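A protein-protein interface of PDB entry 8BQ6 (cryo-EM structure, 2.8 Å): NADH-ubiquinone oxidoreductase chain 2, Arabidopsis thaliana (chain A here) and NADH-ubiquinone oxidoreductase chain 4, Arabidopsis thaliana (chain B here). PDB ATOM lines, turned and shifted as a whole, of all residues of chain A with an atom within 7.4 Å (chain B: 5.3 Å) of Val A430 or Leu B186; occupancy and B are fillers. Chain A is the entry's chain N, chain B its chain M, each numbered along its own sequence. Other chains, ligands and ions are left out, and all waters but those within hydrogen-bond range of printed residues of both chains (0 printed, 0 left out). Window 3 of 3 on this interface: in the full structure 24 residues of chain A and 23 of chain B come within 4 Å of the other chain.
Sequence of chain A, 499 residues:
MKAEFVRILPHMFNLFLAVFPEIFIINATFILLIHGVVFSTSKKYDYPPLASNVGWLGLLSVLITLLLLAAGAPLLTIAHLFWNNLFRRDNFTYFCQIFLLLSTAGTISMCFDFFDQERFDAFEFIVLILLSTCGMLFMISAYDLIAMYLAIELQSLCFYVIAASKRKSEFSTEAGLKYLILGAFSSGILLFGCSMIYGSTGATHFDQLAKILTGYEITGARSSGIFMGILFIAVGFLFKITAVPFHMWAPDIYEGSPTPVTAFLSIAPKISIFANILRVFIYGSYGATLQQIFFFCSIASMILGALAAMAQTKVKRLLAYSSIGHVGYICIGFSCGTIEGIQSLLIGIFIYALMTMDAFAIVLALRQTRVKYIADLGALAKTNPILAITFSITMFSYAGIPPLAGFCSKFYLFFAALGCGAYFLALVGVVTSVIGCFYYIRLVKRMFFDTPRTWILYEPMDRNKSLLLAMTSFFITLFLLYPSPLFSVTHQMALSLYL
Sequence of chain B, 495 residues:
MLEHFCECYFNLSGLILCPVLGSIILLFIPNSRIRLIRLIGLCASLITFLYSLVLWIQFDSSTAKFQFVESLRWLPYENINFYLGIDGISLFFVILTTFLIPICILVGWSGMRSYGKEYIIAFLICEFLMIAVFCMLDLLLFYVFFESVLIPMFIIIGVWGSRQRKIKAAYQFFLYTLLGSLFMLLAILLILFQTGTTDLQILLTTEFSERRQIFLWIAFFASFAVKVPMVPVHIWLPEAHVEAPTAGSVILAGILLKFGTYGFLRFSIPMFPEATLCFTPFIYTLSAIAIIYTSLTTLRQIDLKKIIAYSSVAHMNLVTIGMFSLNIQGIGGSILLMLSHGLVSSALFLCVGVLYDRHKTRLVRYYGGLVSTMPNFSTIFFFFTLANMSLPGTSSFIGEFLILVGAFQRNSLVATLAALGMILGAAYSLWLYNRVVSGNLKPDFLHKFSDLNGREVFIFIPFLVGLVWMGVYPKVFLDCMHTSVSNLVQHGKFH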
ATOM      1  N   MET A 302      36.412 -21.874   9.442  1.00  0.00           N
ATOM      2  CA  MET A 302      35.601 -21.784  10.653  1.00  0.00           C
ATOM      3  C   MET A 302      36.462 -21.446  11.864  1.00  0.00           C
ATOM      4  O   MET A 302      36.187 -20.478  12.588  1.00  0.00           O
ATOM      5  CB  MET A 302      34.844 -23.089  10.878  1.00  0.00           C
ATOM      6  CG  MET A 302      33.607 -23.241  10.025  1.00  0.00           C
ATOM      7  SD  MET A 302      32.719 -24.767  10.382  1.00  0.00           S
ATOM      8  CE  MET A 302      33.970 -25.984  10.004  1.00  0.00           C
ATOM      9  N   TYR A 329      31.313 -22.430   6.831  1.00  0.00           N
ATOM     10  CA  TYR A 329      30.098 -23.216   7.055  1.00  0.00           C
ATOM     11  C   TYR A 329      29.419 -23.587   5.738  1.00  0.00           C
ATOM     12  O   TYR A 329      28.964 -24.725   5.567  1.00  0.00           O
ATOM     13  CB  TYR A 329      29.112 -22.469   7.956  1.00  0.00           C
ATOM     14  CG  TYR A 329      29.606 -22.203   9.358  1.00  0.00           C
ATOM     15  CD1 TYR A 329      30.102 -20.965   9.706  1.00  0.00           C
ATOM     16  CD2 TYR A 329      29.560 -23.185  10.334  1.00  0.00           C
ATOM     17  CE1 TYR A 329      30.562 -20.705  10.972  1.00  0.00           C
ATOM     18  CE2 TYR A 329      30.014 -22.933  11.616  1.00  0.00           C
ATOM     19  CZ  TYR A 329      30.515 -21.688  11.927  1.00  0.00           C
ATOM     20  OH  TYR A 329      30.971 -21.416  13.194  1.00  0.00           O
ATOM     21  N   LEU A 413      24.930 -27.643   8.970  1.00  0.00           N
ATOM     22  CA  LEU A 413      26.309 -28.001   9.279  1.00  0.00           C
ATOM     23  C   LEU A 413      26.337 -29.324  10.022  1.00  0.00           C
ATOM     24  O   LEU A 413      27.016 -30.276   9.613  1.00  0.00           O
ATOM     25  CB  LEU A 413      26.977 -26.907  10.117  1.00  0.00           C
ATOM     26  CG  LEU A 413      28.510 -26.792  10.167  1.00  0.00           C
ATOM     27  CD1 LEU A 413      29.191 -27.982  10.834  1.00  0.00           C
ATOM     28  CD2 LEU A 413      29.085 -26.569   8.786  1.00  0.00           C
ATOM     29  N   PHE A 414      25.519 -29.431  11.067  1.00  0.00           N
ATOM     30  CA  PHE A 414      25.537 -30.669  11.887  1.00  0.00           C
ATOM     31  C   PHE A 414      24.815 -31.795  11.141  1.00  0.00           C
ATOM     32  O   PHE A 414      25.198 -32.947  11.341  1.00  0.00           O
ATOM     33  CB  PHE A 414      24.978 -30.384  13.285  1.00  0.00           C
ATOM     34  CG  PHE A 414      25.813 -29.403  14.064  1.00  0.00           C
ATOM     35  CD1 PHE A 414      25.222 -28.404  14.816  1.00  0.00           C
ATOM     36  CD2 PHE A 414      27.197 -29.465  14.024  1.00  0.00           C
ATOM     37  CE1 PHE A 414      25.994 -27.500  15.527  1.00  0.00           C
ATOM     38  CE2 PHE A 414      27.967 -28.555  14.730  1.00  0.00           C
ATOM     39  CZ  PHE A 414      27.363 -27.574  15.480  1.00  0.00           C
ATOM     40  N   PHE A 415      23.828 -31.471  10.301  1.00  0.00           N
ATOM     41  CA  PHE A 415      23.149 -32.500   9.524  1.00  0.00           C
ATOM     42  C   PHE A 415      24.099 -33.188   8.552  1.00  0.00           C
ATOM     43  O   PHE A 415      24.098 -34.417   8.439  1.00  0.00           O
ATOM     44  CB  PHE A 415      21.963 -31.885   8.789  1.00  0.00           C
ATOM     45  CG  PHE A 415      20.914 -32.874   8.412  1.00  0.00           C
ATOM     46  CD1 PHE A 415      20.671 -33.980   9.202  1.00  0.00           C
ATOM     47  CD2 PHE A 415      20.153 -32.688   7.278  1.00  0.00           C
ATOM     48  CE1 PHE A 415      19.704 -34.893   8.850  1.00  0.00           C
ATOM     49  CE2 PHE A 415      19.183 -33.595   6.927  1.00  0.00           C
ATOM     50  CZ  PHE A 415      18.957 -34.697   7.712  1.00  0.00           C
ATOM     51  N   ALA A 417      27.434 -33.114   8.889  1.00  0.00           N
ATOM     52  CA  ALA A 417      28.495 -33.720   9.687  1.00  0.00           C
ATOM     53  C   ALA A 417      28.104 -35.113  10.161  1.00  0.00           C
ATOM     54  O   ALA A 417      28.946 -36.016  10.218  1.00  0.00           O
ATOM     55  CB  ALA A 417      28.835 -32.827  10.877  1.00  0.00           C
ATOM     56  N   LEU A 418      26.815 -35.294  10.450  1.00  0.00           N
ATOM     57  CA  LEU A 418      26.316 -36.623  10.894  1.00  0.00           C
ATOM     58  C   LEU A 418      25.783 -37.399   9.684  1.00  0.00           C
ATOM     59  O   LEU A 418      25.425 -38.573   9.859  1.00  0.00           O
ATOM     60  CB  LEU A 418      25.247 -36.382  11.961  1.00  0.00           C
ATOM     61  CG  LEU A 418      25.726 -35.577  13.168  1.00  0.00           C
ATOM     62  CD1 LEU A 418      24.556 -35.106  14.007  1.00  0.00           C
ATOM     63  CD2 LEU A 418      26.717 -36.363  14.012  1.00  0.00           C
ATOM     64  N   TYR A 423      32.741 -36.593  12.537  1.00  0.00           N
ATOM     65  CA  TYR A 423      32.546 -36.087  13.890  1.00  0.00           C
ATOM     66  C   TYR A 423      33.569 -35.046  14.304  1.00  0.00           C
ATOM     67  O   TYR A 423      33.285 -34.243  15.196  1.00  0.00           O
ATOM     68  CB  TYR A 423      32.564 -37.237  14.898  1.00  0.00           C
ATOM     69  CG  TYR A 423      31.857 -38.439  14.357  1.00  0.00           C
ATOM     70  CD1 TYR A 423      30.566 -38.329  13.871  1.00  0.00           C
ATOM     71  CD2 TYR A 423      32.473 -39.679  14.320  1.00  0.00           C
ATOM     72  CE1 TYR A 423      29.912 -39.408  13.356  1.00  0.00           C
ATOM     73  CE2 TYR A 423      31.820 -40.775  13.810  1.00  0.00           C
ATOM     74  CZ  TYR A 423      30.539 -40.631  13.328  1.00  0.00           C
ATOM     75  OH  TYR A 423      29.868 -41.710  12.812  1.00  0.00           O
ATOM     76  N   PHE A 424      34.756 -35.048  13.699  1.00  0.00           N
ATOM     77  CA  PHE A 424      35.689 -33.957  13.949  1.00  0.00           C
ATOM     78  C   PHE A 424      35.144 -32.647  13.403  1.00  0.00           C
ATOM     79  O   PHE A 424      35.292 -31.589  14.029  1.00  0.00           O
ATOM     80  CB  PHE A 424      37.047 -34.269  13.337  1.00  0.00           C
ATOM     81  CG  PHE A 424      38.005 -33.128  13.415  1.00  0.00           C
ATOM     82  CD1 PHE A 424      38.489 -32.698  14.637  1.00  0.00           C
ATOM     83  CD2 PHE A 424      38.405 -32.465  12.271  1.00  0.00           C
ATOM     84  CE1 PHE A 424      39.364 -31.641  14.714  1.00  0.00           C
ATOM     85  CE2 PHE A 424      39.283 -31.407  12.343  1.00  0.00           C
ATOM     86  CZ  PHE A 424      39.764 -30.994  13.567  1.00  0.00           C
ATOM     87  N   LEU A 425      34.508 -32.700  12.234  1.00  0.00           N
ATOM     88  CA  LEU A 425      33.797 -31.536  11.728  1.00  0.00           C
ATOM     89  C   LEU A 425      32.710 -31.091  12.698  1.00  0.00           C
ATOM     90  O   LEU A 425      32.525 -29.891  12.923  1.00  0.00           O
ATOM     91  CB  LEU A 425      33.194 -31.851  10.365  1.00  0.00           C
ATOM     92  CG  LEU A 425      32.512 -30.650   9.732  1.00  0.00           C
ATOM     93  CD1 LEU A 425      33.544 -29.567   9.523  1.00  0.00           C
ATOM     94  CD2 LEU A 425      31.853 -31.060   8.438  1.00  0.00           C
ATOM     95  N   ALA A 426      31.974 -32.057  13.252  1.00  0.00           N
ATOM     96  CA  ALA A 426      30.910 -31.728  14.231  1.00  0.00           C
ATOM     97  C   ALA A 426      31.522 -31.023  15.445  1.00  0.00           C
ATOM     98  O   ALA A 426      30.983 -29.980  15.823  1.00  0.00           O
ATOM     99  CB  ALA A 426      30.150 -32.970  14.616  1.00  0.00           C
ATOM    100  N   LEU A 427      32.616 -31.550  16.002  1.00  0.00           N
ATOM    101  CA  LEU A 427      33.278 -30.930  17.147  1.00  0.00           C
ATOM    102  C   LEU A 427      33.770 -29.522  16.823  1.00  0.00           C
ATOM    103  O   LEU A 427      33.601 -28.593  17.630  1.00  0.00           O
ATOM    104  CB  LEU A 427      34.432 -31.817  17.616  1.00  0.00           C
ATOM    105  CG  LEU A 427      35.462 -31.220  18.576  1.00  0.00           C
ATOM    106  CD1 LEU A 427      34.959 -31.181  20.006  1.00  0.00           C
ATOM    107  CD2 LEU A 427      36.748 -32.021  18.492  1.00  0.00           C
ATOM    108  N   VAL A 428      34.391 -29.343  15.655  1.00  0.00           N
ATOM    109  CA  VAL A 428      34.815 -28.005  15.252  1.00  0.00           C
ATOM    110  C   VAL A 428      33.615 -27.074  15.171  1.00  0.00           C
ATOM    111  O   VAL A 428      33.676 -25.920  15.611  1.00  0.00           O
ATOM    112  CB  VAL A 428      35.590 -28.052  13.923  1.00  0.00           C
ATOM    113  CG1 VAL A 428      35.817 -26.647  13.401  1.00  0.00           C
ATOM    114  CG2 VAL A 428      36.924 -28.734  14.123  1.00  0.00           C
ATOM    115  N   GLY A 429      32.507 -27.560  14.611  1.00  0.00           N
ATOM    116  CA  GLY A 429      31.313 -26.738  14.512  1.00  0.00           C
ATOM    117  C   GLY A 429      30.771 -26.320  15.865  1.00  0.00           C
ATOM    118  O   GLY A 429      30.407 -25.161  16.061  1.00  0.00           O
ATOM    119  N   VAL A 430      30.734 -27.251  16.812  1.00  0.00           N
ATOM    120  CA  VAL A 430      30.239 -26.936  18.184  1.00  0.00           C
ATOM    121  C   VAL A 430      31.151 -25.883  18.822  1.00  0.00           C
ATOM    122  O   VAL A 430      30.612 -24.913  19.358  1.00  0.00           O
ATOM    123  CB  VAL A 430      30.119 -28.217  19.035  1.00  0.00           C
ATOM    124  CG1 VAL A 430      30.113 -27.942  20.531  1.00  0.00           C
ATOM    125  CG2 VAL A 430      28.904 -29.041  18.645  1.00  0.00           C
ATOM    126  N   VAL A 431      32.473 -26.039  18.741  1.00  0.00           N
ATOM    127  CA  VAL A 431      33.361 -25.113  19.441  1.00  0.00           C
ATOM    128  C   VAL A 431      33.322 -23.736  18.781  1.00  0.00           C
ATOM    129  O   VAL A 431      33.229 -22.701  19.459  1.00  0.00           O
ATOM    130  CB  VAL A 431      34.792 -25.673  19.499  1.00  0.00           C
ATOM    131  CG1 VAL A 431      35.723 -24.654  20.134  1.00  0.00           C
ATOM    132  CG2 VAL A 431      34.822 -27.002  20.240  1.00  0.00           C
ATOM    133  N   THR A 432      33.379 -23.699  17.447  1.00  0.00           N
ATOM    134  CA  THR A 432      33.388 -22.417  16.755  1.00  0.00           C
ATOM    135  C   THR A 432      32.038 -21.718  16.837  1.00  0.00           C
ATOM    136  O   THR A 432      31.992 -20.487  16.867  1.00  0.00           O
ATOM    137  CB  THR A 432      33.807 -22.591  15.295  1.00  0.00           C
ATOM    138  OG1 THR A 432      32.990 -23.585  14.666  1.00  0.00           O
ATOM    139  CG2 THR A 432      35.258 -23.000  15.208  1.00  0.00           C
ATOM    140  N   SER A 433      30.938 -22.472  16.887  1.00  0.00           N
ATOM    141  CA  SER A 433      29.640 -21.860  17.129  1.00  0.00           C
ATOM    142  C   SER A 433      29.599 -21.195  18.495  1.00  0.00           C
ATOM    143  O   SER A 433      29.064 -20.091  18.639  1.00  0.00           O
ATOM    144  CB  SER A 433      28.535 -22.908  17.021  1.00  0.00           C
ATOM    145  OG  SER A 433      28.198 -23.166  15.673  1.00  0.00           O
ATOM    146  N   VAL A 434      30.153 -21.854  19.515  1.00  0.00           N
ATOM    147  CA  VAL A 434      30.176 -21.231  20.836  1.00  0.00           C
ATOM    148  C   VAL A 434      31.014 -19.951  20.815  1.00  0.00           C
ATOM    149  O   VAL A 434      30.612 -18.915  21.368  1.00  0.00           O
ATOM    150  CB  VAL A 434      30.683 -22.237  21.885  1.00  0.00           C
ATOM    151  CG1 VAL A 434      30.945 -21.542  23.204  1.00  0.00           C
ATOM    152  CG2 VAL A 434      29.681 -23.365  22.062  1.00  0.00           C
ATOM    153  N   ILE A 435      32.184 -19.996  20.174  1.00  0.00           N
ATOM    154  CA  ILE A 435      33.035 -18.807  20.101  1.00  0.00           C
ATOM    155  C   ILE A 435      32.320 -17.672  19.370  1.00  0.00           C
ATOM    156  O   ILE A 435      32.358 -16.504  19.796  1.00  0.00           O
ATOM    157  CB  ILE A 435      34.373 -19.151  19.426  1.00  0.00           C
ATOM    158  CG1 ILE A 435      35.170 -20.117  20.296  1.00  0.00           C
ATOM    159  CG2 ILE A 435      35.170 -17.889  19.158  1.00  0.00           C
ATOM    160  CD1 ILE A 435      36.242 -20.852  19.545  1.00  0.00           C
ATOM    161  N   GLY A 436      31.675 -17.996  18.247  1.00  0.00           N
ATOM    162  CA  GLY A 436      30.929 -16.992  17.516  1.00  0.00           C
ATOM    163  C   GLY A 436      29.818 -16.389  18.346  1.00  0.00           C
ATOM    164  O   GLY A 436      29.634 -15.170  18.357  1.00  0.00           O
ATOM    165  N   CYS A 437      29.068 -17.232  19.054  1.00  0.00           N
ATOM    166  CA  CYS A 437      28.030 -16.732  19.943  1.00  0.00           C
ATOM    167  C   CYS A 437      28.603 -15.739  20.940  1.00  0.00           C
ATOM    168  O   CYS A 437      27.998 -14.692  21.199  1.00  0.00           O
ATOM    169  CB  CYS A 437      27.363 -17.898  20.668  1.00  0.00           C
ATOM    170  SG  CYS A 437      26.462 -19.021  19.594  1.00  0.00           S
ATOM    171  N   LEU B 179      26.200 -24.420  24.809  1.00  0.00           N
ATOM    172  CA  LEU B 179      26.964 -25.656  24.653  1.00  0.00           C
ATOM    173  C   LEU B 179      26.081 -26.882  24.857  1.00  0.00           C
ATOM    174  O   LEU B 179      26.062 -27.813  24.027  1.00  0.00           O
ATOM    175  CB  LEU B 179      28.119 -25.664  25.648  1.00  0.00           C
ATOM    176  CG  LEU B 179      29.256 -26.658  25.445  1.00  0.00           C
ATOM    177  CD1 LEU B 179      29.874 -26.490  24.070  1.00  0.00           C
ATOM    178  CD2 LEU B 179      30.285 -26.444  26.530  1.00  0.00           C
ATOM    179  N   LEU B 182      23.664 -27.559  22.156  1.00  0.00           N
ATOM    180  CA  LEU B 182      24.333 -27.977  20.892  1.00  0.00           C
ATOM    181  C   LEU B 182      24.516 -29.499  20.869  1.00  0.00           C
ATOM    182  O   LEU B 182      24.350 -30.081  19.789  1.00  0.00           O
ATOM    183  CB  LEU B 182      25.671 -27.243  20.752  1.00  0.00           C
ATOM    184  CG  LEU B 182      25.577 -25.849  20.135  1.00  0.00           C
ATOM    185  CD1 LEU B 182      26.954 -25.245  19.928  1.00  0.00           C
ATOM    186  CD2 LEU B 182      24.805 -25.882  18.827  1.00  0.00           C
ATOM    187  N   PHE B 183      24.835 -30.115  22.009  1.00  0.00           N
ATOM    188  CA  PHE B 183      24.944 -31.599  22.088  1.00  0.00           C
ATOM    189  C   PHE B 183      23.569 -32.235  21.880  1.00  0.00           C
ATOM    190  O   PHE B 183      23.509 -33.272  21.205  1.00  0.00           O
ATOM    191  CB  PHE B 183      25.568 -32.036  23.415  1.00  0.00           C
ATOM    192  CG  PHE B 183      26.940 -31.466  23.657  1.00  0.00           C
ATOM    193  CD1 PHE B 183      27.926 -31.562  22.689  1.00  0.00           C
ATOM    194  CD2 PHE B 183      27.243 -30.820  24.843  1.00  0.00           C
ATOM    195  CE1 PHE B 183      29.189 -31.035  22.907  1.00  0.00           C
ATOM    196  CE2 PHE B 183      28.508 -30.299  25.064  1.00  0.00           C
ATOM    197  CZ  PHE B 183      29.478 -30.406  24.095  1.00  0.00           C
ATOM    198  N   MET B 184      22.510 -31.636  22.425  1.00  0.00           N
ATOM    199  CA  MET B 184      21.140 -32.153  22.173  1.00  0.00           C
ATOM    200  C   MET B 184      20.860 -32.120  20.673  1.00  0.00           C
ATOM    201  O   MET B 184      20.277 -33.097  20.189  1.00  0.00           O
ATOM    202  CB  MET B 184      20.062 -31.327  22.873  1.00  0.00           C
ATOM    203  CG  MET B 184      18.930 -32.165  23.426  1.00  0.00           C
ATOM    204  SD  MET B 184      17.369 -31.253  23.451  1.00  0.00           S
ATOM    205  CE  MET B 184      17.867 -29.788  24.353  1.00  0.00           C
ATOM    206  N   LEU B 185      21.233 -31.032  19.985  1.00  0.00           N
ATOM    207  CA  LEU B 185      20.959 -30.899  18.530  1.00  0.00           C
ATOM    208  C   LEU B 185      21.589 -32.083  17.798  1.00  0.00           C
ATOM    209  O   LEU B 185      20.900 -32.668  16.955  1.00  0.00           O
ATOM    210  CB  LEU B 185      21.522 -29.572  18.014  1.00  0.00           C
ATOM    211  CG  LEU B 185      21.307 -29.297  16.524  1.00  0.00           C
ATOM    212  CD1 LEU B 185      19.834 -29.368  16.152  1.00  0.00           C
ATOM    213  CD2 LEU B 185      21.888 -27.951  16.130  1.00  0.00           C
ATOM    214  N   LEU B 186      22.845 -32.405  18.109  1.00  0.00           N
ATOM    215  CA  LEU B 186      23.553 -33.526  17.446  1.00  0.00           C
ATOM    216  C   LEU B 186      22.731 -34.806  17.610  1.00  0.00           C
ATOM    217  O   LEU B 186      22.468 -35.449  16.598  1.00  0.00           O
ATOM    218  CB  LEU B 186      24.937 -33.668  18.081  1.00  0.00           C
ATOM    219  CG  LEU B 186      25.896 -32.507  17.823  1.00  0.00           C
ATOM    220  CD1 LEU B 186      27.098 -32.586  18.750  1.00  0.00           C
ATOM    221  CD2 LEU B 186      26.347 -32.482  16.372  1.00  0.00           C
ATOM    222  N   ALA B 187      22.304 -35.122  18.834  1.00  0.00           N
ATOM    223  CA  ALA B 187      21.478 -36.321  19.089  1.00  0.00           C
ATOM    224  C   ALA B 187      20.159 -36.260  18.310  1.00  0.00           C
ATOM    225  O   ALA B 187      19.775 -37.300  17.779  1.00  0.00           O
ATOM    226  CB  ALA B 187      21.225 -36.472  20.567  1.00  0.00           C
ATOM    227  N   ILE B 188      19.486 -35.108  18.278  1.00  0.00           N
ATOM    228  CA  ILE B 188      18.207 -34.956  17.519  1.00  0.00           C
ATOM    229  C   ILE B 188      18.460 -35.296  16.046  1.00  0.00           C
ATOM    230  O   ILE B 188      17.646 -36.035  15.477  1.00  0.00           O
ATOM    231  CB  ILE B 188      17.615 -33.545  17.711  1.00  0.00           C
ATOM    232  CG1 ILE B 188      16.996 -33.404  19.103  1.00  0.00           C
ATOM    233  CG2 ILE B 188      16.615 -33.186  16.625  1.00  0.00           C
ATOM    234  CD1 ILE B 188      17.061 -32.007  19.652  1.00  0.00           C
ATOM    235  N   LEU B 189      19.567 -34.816  15.477  1.00  0.00           N
ATOM    236  CA  LEU B 189      19.897 -35.063  14.046  1.00  0.00           C
ATOM    237  C   LEU B 189      20.328 -36.520  13.849  1.00  0.00           C
ATOM    238  O   LEU B 189      20.055 -37.061  12.772  1.00  0.00           O
ATOM    239  CB  LEU B 189      20.981 -34.066  13.645  1.00  0.00           C
ATOM    240  CG  LEU B 189      20.446 -32.659  13.419  1.00  0.00           C
ATOM    241  CD1 LEU B 189      21.555 -31.689  13.070  1.00  0.00           C
ATOM    242  CD2 LEU B 189      19.399 -32.695  12.330  1.00  0.00           C
ATOM    243  N   LEU B 190      20.955 -37.136  14.850  1.00  0.00           N
ATOM    244  CA  LEU B 190      21.291 -38.580  14.775  1.00  0.00           C
ATOM    245  C   LEU B 190      19.996 -39.378  14.896  1.00  0.00           C
ATOM    246  O   LEU B 190      19.873 -40.382  14.178  1.00  0.00           O
ATOM    247  CB  LEU B 190      22.250 -38.946  15.910  1.00  0.00           C
ATOM    248  CG  LEU B 190      23.701 -38.528  15.699  1.00  0.00           C
ATOM    249  CD1 LEU B 190      24.389 -38.284  17.031  1.00  0.00           C
ATOM    250  CD2 LEU B 190      24.453 -39.566  14.888  1.00  0.00           C
ATOM    251  N   ILE B 191      19.082 -38.979  15.791  1.00  0.00           N
ATOM    252  CA  ILE B 191      17.816 -39.699  15.832  1.00  0.00           C
ATOM    253  C   ILE B 191      17.102 -39.576  14.498  1.00  0.00           C
ATOM    254  O   ILE B 191      16.573 -40.556  13.962  1.00  0.00           O
ATOM    255  CB  ILE B 191      16.942 -39.167  16.978  1.00  0.00           C
ATOM    256  CG1 ILE B 191      17.404 -39.738  18.314  1.00  0.00           C
ATOM    257  CG2 ILE B 191      15.491 -39.521  16.734  1.00  0.00           C
ATOM    258  CD1 ILE B 191      16.852 -38.991  19.501  1.00  0.00           C
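Among the printed residues, pairs that only touch across the chains: Leu A418 with Leu B186 (3.3 Å), Phe A415 with Leu B189 (3.6 Å), Phe A414 with Leu B185 (3.6 Å), Phe A414 with Leu B189 (3.7 Å), Val A430 with Leu B182 (3.7 Å), Val A434 with Leu B179 (3.7 Å), Leu A418 with Leu B189 (3.7 Å), Val A430 with Leu B179 (3.8 Å), Phe A414 with Leu B182 (3.9 Å), Phe A414 with Leu B186 (3.9 Å), Leu A418 with Leu B190 (3.9 Å), Val A434 with Leu B182 (3.9 Å) and Val A430 with Leu B186 (3.98 Å).
Printed residues of chain B within 4 Å of Val A430: Leu B179, Leu B182 and Leu B186.
Leu B186 touches just these residues of chain A: Phe A414, Leu A418 and Val A430.
Of the printed residues of chain B, Val A434 touches Leu B179 (3.7 Å) and Leu B182 (3.9 Å).
Of the printed residues of chain A, Leu B189 touches Phe A414 (3.7 Å), Phe A415 (3.6 Å) and Leu A418 (3.7 Å).
Printed residues of chain B within 4 Å of Phe A414: Leu B182, Leu B185, Leu B186 and Leu B189.
Printed residues of chain A within 4 Å of Leu B190: Leu A418.
Of the printed residues of chain B, Phe A415 touches Leu B189 (3.6 Å).
Thr A432 touches none of the printed residues of chain B.
Leu A427 touches none of the printed residues of chain B.
Of the 22 printed residues of chain A, 5 touch a printed residue of chain B.
Hydrophobic or aromatic side chains of chain A that line the printed part of chain B: Phe A414, Phe A415, Leu A418, Val A430 and Val A434.
Of the 11 printed residues of chain B, 6 touch a printed residue of chain A.
Among the printed residues, 13 pairs touch across the chains.
Among the printed residues, no Asp or Glu carboxylate lies within 4 Å of a Lys or Arg side-chain nitrogen of the other chain.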
